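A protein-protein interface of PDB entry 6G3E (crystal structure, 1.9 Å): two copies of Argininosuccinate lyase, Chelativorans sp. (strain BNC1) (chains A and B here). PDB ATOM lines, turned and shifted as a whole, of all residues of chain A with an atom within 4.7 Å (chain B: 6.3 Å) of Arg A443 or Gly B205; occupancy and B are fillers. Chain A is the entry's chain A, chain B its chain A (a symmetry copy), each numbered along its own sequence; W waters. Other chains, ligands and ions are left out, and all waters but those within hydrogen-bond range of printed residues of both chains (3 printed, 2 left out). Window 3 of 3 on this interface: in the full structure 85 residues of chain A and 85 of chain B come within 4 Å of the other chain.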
ATOM      1  N   GLN A 164      24.565  -3.584 -18.956  1.00  0.00           N
ATOM      2  CA  GLN A 164      24.135  -2.577 -19.926  1.00  0.00           C
ATOM      3  C   GLN A 164      24.914  -1.273 -19.749  1.00  0.00           C
ATOM      4  O   GLN A 164      25.583  -1.077 -18.738  1.00  0.00           O
ATOM      5  CB  GLN A 164      22.630  -2.312 -19.796  1.00  0.00           C
ATOM      6  CG  GLN A 164      21.757  -3.516 -20.146  1.00  0.00           C
ATOM      7  CD  GLN A 164      20.285  -3.279 -19.867  1.00  0.00           C
ATOM      8  OE1 GLN A 164      19.899  -2.251 -19.307  1.00  0.00           O
ATOM      9  NE2 GLN A 164      19.452  -4.232 -20.256  1.00  0.00           N
ATOM     10  N   PRO A 165      24.841  -0.373 -20.742  1.00  0.00           N
ATOM     11  CA  PRO A 165      25.478   0.936 -20.577  1.00  0.00           C
ATOM     12  C   PRO A 165      24.714   1.860 -19.644  1.00  0.00           C
ATOM     13  O   PRO A 165      23.487   1.935 -19.715  1.00  0.00           O
ATOM     14  CB  PRO A 165      25.487   1.514 -22.000  1.00  0.00           C
ATOM     15  CG  PRO A 165      25.236   0.352 -22.901  1.00  0.00           C
ATOM     16  CD  PRO A 165      24.375  -0.576 -22.124  1.00  0.00           C
ATOM     17  N   THR A 368      20.966  -5.931 -25.354  1.00  0.00           N
ATOM     18  CA  THR A 368      19.562  -5.794 -24.978  1.00  0.00           C
ATOM     19  C   THR A 368      18.858  -4.839 -25.940  1.00  0.00           C
ATOM     20  O   THR A 368      17.734  -5.097 -26.375  1.00  0.00           O
ATOM     21  CB  THR A 368      19.379  -5.280 -23.537  1.00  0.00           C
ATOM     22  OG1 THR A 368      19.936  -6.220 -22.613  1.00  0.00           O
ATOM     23  CG2 THR A 368      17.899  -5.101 -23.217  1.00  0.00           C
ATOM     24  N   ASP A 369      19.520  -3.739 -26.278  1.00  0.00           N
ATOM     25  CA  ASP A 369      18.924  -2.766 -27.186  1.00  0.00           C
ATOM     26  C   ASP A 369      18.775  -3.344 -28.586  1.00  0.00           C
ATOM     27  O   ASP A 369      17.834  -2.993 -29.294  1.00  0.00           O
ATOM     28  CB  ASP A 369      19.741  -1.480 -27.237  1.00  0.00           C
ATOM     29  CG  ASP A 369      19.314  -0.481 -26.180  1.00  0.00           C
ATOM     30  OD1 ASP A 369      18.692  -0.898 -25.180  1.00  0.00           O
ATOM     31  OD2 ASP A 369      19.610   0.724 -26.336  1.00  0.00           O
ATOM     32  N   ASN A 439      22.250   3.862 -26.243  1.00  0.00           N
ATOM     33  CA  ASN A 439      21.669   3.002 -25.212  1.00  0.00           C
ATOM     34  C   ASN A 439      21.310   3.831 -23.990  1.00  0.00           C
ATOM     35  O   ASN A 439      20.234   3.677 -23.416  1.00  0.00           O
ATOM     36  CB  ASN A 439      22.625   1.877 -24.798  1.00  0.00           C
ATOM     37  CG  ASN A 439      22.518   0.645 -25.677  1.00  0.00           C
ATOM     38  OD1 ASN A 439      22.238  -0.453 -25.192  1.00  0.00           O
ATOM     39  ND2 ASN A 439      22.753   0.815 -26.974  1.00  0.00           N
ATOM     40  N   VAL A 440      22.226   4.710 -23.600  1.00  0.00           N
ATOM     41  CA  VAL A 440      22.024   5.578 -22.448  1.00  0.00           C
ATOM     42  C   VAL A 440      20.876   6.557 -22.709  1.00  0.00           C
ATOM     43  O   VAL A 440      19.993   6.731 -21.865  1.00  0.00           O
ATOM     44  CB  VAL A 440      23.324   6.352 -22.097  1.00  0.00           C
ATOM     45  CG1 VAL A 440      23.063   7.453 -21.078  1.00  0.00           C
ATOM     46  CG2 VAL A 440      24.381   5.392 -21.568  1.00  0.00           C
ATOM     47  N   LEU A 441      20.878   7.185 -23.880  1.00  0.00           N
ATOM     48  CA  LEU A 441      19.862   8.187 -24.196  1.00  0.00           C
ATOM     49  C   LEU A 441      18.456   7.581 -24.271  1.00  0.00           C
ATOM     50  O   LEU A 441      17.489   8.226 -23.875  1.00  0.00           O
ATOM     51  CB  LEU A 441      20.198   8.898 -25.511  1.00  0.00           C
ATOM     52  CG  LEU A 441      21.463   9.769 -25.530  1.00  0.00           C
ATOM     53  CD1 LEU A 441      21.616  10.437 -26.894  1.00  0.00           C
ATOM     54  CD2 LEU A 441      21.462  10.818 -24.428  1.00  0.00           C
ATOM     55  N   ARG A 442      18.340   6.350 -24.767  1.00  0.00           N
ATOM     56  CA  ARG A 442      17.042   5.671 -24.836  1.00  0.00           C
ATOM     57  C   ARG A 442      16.440   5.440 -23.457  1.00  0.00           C
ATOM     58  O   ARG A 442      15.221   5.452 -23.289  1.00  0.00           O
ATOM     59  CB  ARG A 442      17.168   4.325 -25.542  1.00  0.00           C
ATOM     60  CG  ARG A 442      17.061   4.400 -27.046  1.00  0.00           C
ATOM     61  CD  ARG A 442      17.608   3.136 -27.705  1.00  0.00           C
ATOM     62  NE  ARG A 442      18.219   3.493 -28.975  1.00  0.00           N
ATOM     63  CZ  ARG A 442      19.395   3.064 -29.407  1.00  0.00           C
ATOM     64  NH1 ARG A 442      20.126   2.215 -28.697  1.00  0.00           N
ATOM     65  NH2 ARG A 442      19.830   3.482 -30.580  1.00  0.00           N
ATOM     66  N   ARG A 443      17.305   5.208 -22.477  1.00  0.00           N
ATOM     67  CA  ARG A 443      16.866   4.903 -21.122  1.00  0.00           C
ATOM     68  C   ARG A 443      16.599   6.188 -20.346  1.00  0.00           C
ATOM     69  O   ARG A 443      17.413   6.610 -19.520  1.00  0.00           O
ATOM     70  CB  ARG A 443      17.912   4.041 -20.417  1.00  0.00           C
ATOM     71  CG  ARG A 443      17.961   2.625 -20.960  1.00  0.00           C
ATOM     72  CD  ARG A 443      19.235   1.872 -20.584  1.00  0.00           C
ATOM     73  NE  ARG A 443      19.098   0.458 -20.919  1.00  0.00           N
ATOM     74  CZ  ARG A 443      19.147  -0.018 -22.159  1.00  0.00           C
ATOM     75  NH1 ARG A 443      18.994  -1.319 -22.384  1.00  0.00           N
ATOM     76  NH2 ARG A 443      19.335   0.810 -23.181  1.00  0.00           N
ATOM     77  N   GLU A 444      15.443   6.796 -20.606  1.00  0.00           N
ATOM     78  CA  GLU A 444      15.159   8.154 -20.145  1.00  0.00           C
ATOM     79  C   GLU A 444      13.995   8.267 -19.150  1.00  0.00           C
ATOM     80  O   GLU A 444      13.508   9.365 -18.887  1.00  0.00           O
ATOM     81  CB  GLU A 444      14.870   9.048 -21.353  1.00  0.00           C
ATOM     82  CG  GLU A 444      13.607   8.654 -22.111  1.00  0.00           C
ATOM     83  CD  GLU A 444      13.308   9.579 -23.275  1.00  0.00           C
ATOM     84  OE1 GLU A 444      13.533  10.803 -23.142  1.00  0.00           O
ATOM     85  OE2 GLU A 444      12.849   9.079 -24.325  1.00  0.00           O
ATOM     86  N   GLY A 445      13.556   7.148 -18.591  1.00  0.00           N
ATOM     87  CA  GLY A 445      12.529   7.176 -17.563  1.00  0.00           C
ATOM     88  C   GLY A 445      13.070   7.577 -16.198  1.00  0.00           C
ATOM     89  O   GLY A 445      14.255   7.891 -16.053  1.00  0.00           O
ATOM     90  N   MET A 448      16.626   6.272 -14.517  1.00  0.00           N
ATOM     91  CA  MET A 448      17.393   5.634 -15.582  1.00  0.00           C
ATOM     92  C   MET A 448      18.594   6.520 -15.968  1.00  0.00           C
ATOM     93  O   MET A 448      18.643   7.691 -15.596  1.00  0.00           O
ATOM     94  CB  MET A 448      16.479   5.359 -16.779  1.00  0.00           C
ATOM     95  CG  MET A 448      15.260   4.526 -16.421  1.00  0.00           C
ATOM     96  SD  MET A 448      14.334   3.983 -17.869  1.00  0.00           S
ATOM     97  CE  MET A 448      12.943   3.143 -17.095  1.00  0.00           C
ATOM     98  N   PRO A 449      19.580   5.956 -16.691  1.00  0.00           N
ATOM     99  CA  PRO A 449      20.855   6.673 -16.852  1.00  0.00           C
ATOM    100  C   PRO A 449      20.894   7.873 -17.812  1.00  0.00           C
ATOM    101  O   PRO A 449      21.926   8.542 -17.829  1.00  0.00           O
ATOM    102  CB  PRO A 449      21.800   5.584 -17.371  1.00  0.00           C
ATOM    103  CG  PRO A 449      20.924   4.557 -17.970  1.00  0.00           C
ATOM    104  CD  PRO A 449      19.671   4.563 -17.163  1.00  0.00           C
ATOM    105  N   ALA A 450      19.850   8.140 -18.591  1.00  0.00           N
ATOM    106  CA  ALA A 450      19.891   9.293 -19.496  1.00  0.00           C
ATOM    107  C   ALA A 450      20.216  10.565 -18.706  1.00  0.00           C
ATOM    108  O   ALA A 450      19.696  10.749 -17.610  1.00  0.00           O
ATOM    109  CB  ALA A 450      18.572   9.451 -20.234  1.00  0.00           C
ATOM    110  N   SER A 453      17.474  12.427 -16.937  1.00  0.00           N
ATOM    111  CA  SER A 453      16.888  11.691 -15.819  1.00  0.00           C
ATOM    112  C   SER A 453      17.781  11.750 -14.580  1.00  0.00           C
ATOM    113  O   SER A 453      17.302  11.962 -13.467  1.00  0.00           O
ATOM    114  CB  SER A 453      16.638  10.237 -16.203  1.00  0.00           C
ATOM    115  OG  SER A 453      15.816  10.150 -17.350  1.00  0.00           O
ATOM    116  N   GLY B 109      10.585  -4.862 -21.383  1.00  0.00           N
ATOM    117  CA  GLY B 109      10.923  -3.835 -20.413  1.00  0.00           C
ATOM    118  C   GLY B 109      11.129  -4.347 -18.994  1.00  0.00           C
ATOM    119  O   GLY B 109      11.110  -3.563 -18.044  1.00  0.00           O
ATOM    120  N   GLY B 199      10.456  -1.562 -13.318  1.00  0.00           N
ATOM    121  CA  GLY B 199      10.851  -0.548 -14.277  1.00  0.00           C
ATOM    122  C   GLY B 199      12.358  -0.387 -14.293  1.00  0.00           C
ATOM    123  O   GLY B 199      12.920   0.196 -15.219  1.00  0.00           O
ATOM    124  N   ALA B 200      13.017  -0.905 -13.261  1.00  0.00           N
ATOM    125  CA  ALA B 200      14.472  -0.959 -13.238  1.00  0.00           C
ATOM    126  C   ALA B 200      14.975  -1.964 -14.267  1.00  0.00           C
ATOM    127  O   ALA B 200      16.107  -1.862 -14.748  1.00  0.00           O
ATOM    128  CB  ALA B 200      14.969  -1.330 -11.848  1.00  0.00           C
ATOM    129  N   ALA B 201      14.120  -2.931 -14.598  1.00  0.00           N
ATOM    130  CA  ALA B 201      14.480  -4.024 -15.491  1.00  0.00           C
ATOM    131  C   ALA B 201      15.742  -4.726 -14.970  1.00  0.00           C
ATOM    132  O   ALA B 201      15.778  -5.140 -13.809  1.00  0.00           O
ATOM    133  CB  ALA B 201      14.670  -3.512 -16.916  1.00  0.00           C
ATOM    134  N   ALA B 202      16.770  -4.862 -15.805  1.00  0.00           N
ATOM    135  CA  ALA B 202      17.973  -5.586 -15.394  1.00  0.00           C
ATOM    136  C   ALA B 202      18.712  -4.855 -14.279  1.00  0.00           C
ATOM    137  O   ALA B 202      19.234  -5.488 -13.361  1.00  0.00           O
ATOM    138  CB  ALA B 202      18.899  -5.800 -16.585  1.00  0.00           C
ATOM    139  N   THR B 203      18.719  -3.544 -14.347  1.00  0.00           N
ATOM    140  CA  THR B 203      19.480  -2.677 -13.482  1.00  0.00           C
ATOM    141  C   THR B 203      19.635  -1.255 -14.021  1.00  0.00           C
ATOM    142  O   THR B 203      20.102  -0.450 -13.330  1.00  0.00           O
ATOM    143  CB  THR B 203      20.907  -3.201 -13.246  1.00  0.00           C
ATOM    144  OG1 THR B 203      21.601  -2.370 -12.331  1.00  0.00           O
ATOM    145  CG2 THR B 203      21.605  -3.366 -14.538  1.00  0.00           C
ATOM    146  N   ALA B 204      19.263  -1.032 -15.272  1.00  0.00           N
ATOM    147  CA  ALA B 204      19.492   0.244 -15.944  1.00  0.00           C
ATOM    148  C   ALA B 204      18.242   0.773 -16.645  1.00  0.00           C
ATOM    149  O   ALA B 204      18.327   1.660 -17.495  1.00  0.00           O
ATOM    150  CB  ALA B 204      20.620   0.101 -16.946  1.00  0.00           C
ATOM    151  N   GLY B 205      17.083   0.242 -16.285  1.00  0.00           N
ATOM    152  CA  GLY B 205      15.852   0.631 -16.944  1.00  0.00           C
ATOM    153  C   GLY B 205      15.758   0.066 -18.350  1.00  0.00           C
ATOM    154  O   GLY B 205      16.271  -1.015 -18.637  1.00  0.00           O
ATOM    155  N   THR B 206      15.106   0.809 -19.235  1.00  0.00           N
ATOM    156  CA  THR B 206      14.759   0.297 -20.556  1.00  0.00           C
ATOM    157  C   THR B 206      14.411   1.439 -21.502  1.00  0.00           C
ATOM    158  O   THR B 206      14.043   2.524 -21.063  1.00  0.00           O
ATOM    159  CB  THR B 206      13.564  -0.673 -20.479  1.00  0.00           C
ATOM    160  OG1 THR B 206      13.216  -1.124 -21.795  1.00  0.00           O
ATOM    161  CG2 THR B 206      12.358   0.011 -19.838  1.00  0.00           C
ATOM    162  N   GLY B 207      14.533   1.184 -22.801  1.00  0.00           N
ATOM    163  CA  GLY B 207      14.134   2.147 -23.809  1.00  0.00           C
ATOM    164  C   GLY B 207      12.630   2.143 -24.020  1.00  0.00           C
ATOM    165  O   GLY B 207      12.066   3.101 -24.548  1.00  0.00           O
ATOM    166  N   SER B 228      17.451   2.912 -10.846  1.00  0.00           N
ATOM    167  CA  SER B 228      17.275   1.548 -11.340  1.00  0.00           C
ATOM    168  C   SER B 228      18.273   0.553 -10.742  1.00  0.00           C
ATOM    169  O   SER B 228      17.954  -0.628 -10.588  1.00  0.00           O
ATOM    170  CB  SER B 228      17.375   1.532 -12.869  1.00  0.00           C
ATOM    171  OG  SER B 228      18.653   1.959 -13.307  1.00  0.00           O
HETATM  172  O   HOH W   1      16.018  -0.520 -24.545  1.00  0.00           O
HETATM  173  O   HOH W   2      11.754   4.327 -20.402  1.00  0.00           O
HETATM  174  O   HOH W   3      16.983  -2.751 -20.652  1.00  0.00           O
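N of Thr B206 sits at hydrogen-bond distance from SD of Met A448 (3.5 Å).
The side-chain amide nitrogen (NE2) of Gln A164 is in hydrogen-bond range of the side-chain hydroxyl (OG1) of Thr A368, 3.1 Å away.
The side-chain amide oxygen (OE1) of Gln A164 lies within hydrogen-bond range of the guanidinium group (NE) of Arg A443 (3.3 Å).
NH2 of Arg A443 lies within salt-bridge range of OD1 of Asp A369 (2.7 Å).
The backbone carbonyl oxygen (O) of Asn A439 lies within hydrogen-bond range of the guanidinium group (NH2) of Arg A443 (3.0 Å).
The backbone carbonyl oxygen (O) of Arg A443 lies within hydrogen-bond range of the backbone NH (N) of Ala A450 (3.0 Å).
SD of Met A448 lies within hydrogen-bond range of N of Gly A445.
Among the printed residues, merely in contact across the chains: Pro A449 with Ala B204 (3.2 Å), Arg A443 with Ala B204 (3.2 Å), Gln A164 with Ala B204 (3.4 Å), Met A448 with Gly B199 (3.5 Å), Arg A442 with Gly B207 (3.5 Å), Arg A443 with Thr B206 (3.7 Å), Met A448 with Gly B205 (3.8 Å), Arg A442 with Thr B206 (3.9 Å), Gln A164 with Gly B205 (3.9 Å) and Arg A443 with Gly B205 (3.9 Å).
Printed residues of chain B within 4 Å of Gln A164: Ala B204 and Gly B205.
Val A440 touches none of the printed residues of chain B.
Of chain B, only Ala B204 (3.2 Å), Gly B205 (3.9 Å) and Thr B206 (3.7 Å) come within 4 Å of Arg A443.
Printed residues of chain B within 4 Å of Met A448: Gly B199 (3.5 Å), Gly B205 (3.8 Å) and Thr B206 (3.5 Å).
Printed residues of chain A within 4 Å of Gly B199: Met A448.
Of the printed residues of chain A, Gly B205 touches Gln A164, Arg A443 and Met A448.
Printed residues of chain A within 4 Å of Gly B207: Arg A442.
The nearest printed residue of chain A that does not touch Gly B205 is Pro A449 (5.1 Å).
The nearest printed residue of chain A that does not touch Ala B204 is Met A448 (4.2 Å).
Of the 15 printed residues of chain A, 5 touch a printed residue of chain B.
Hydrophobic or aromatic side chains of chain A within 4 Å of the printed part of chain B: Met A448 and Pro A449.
Among the printed residues, 11 pairs touch across the chains.
Among the printed residues, no Asp or Glu carboxylate lies within 4 Å of a Lys or Arg side-chain nitrogen of the other chain.
No position is printed for both chains.
Of the 11 pairs that touch across the chains among the printed residues, none has its exchanged pair printed and touching as well.
Water W3 lies within hydrogen-bond range of O of Gly B205, NE2 of Gln A164 and NH1 of Arg A443.
Water W1 lies within hydrogen-bond range of OD1 of Asp A369 (2.8 Å) and N of Gly B207 (2.9 Å).
Water W2 bridges the backbone carbonyl oxygen of Thr B206 (3.0 Å) and the side-chain sulfur of Met A448 (3.6 Å).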
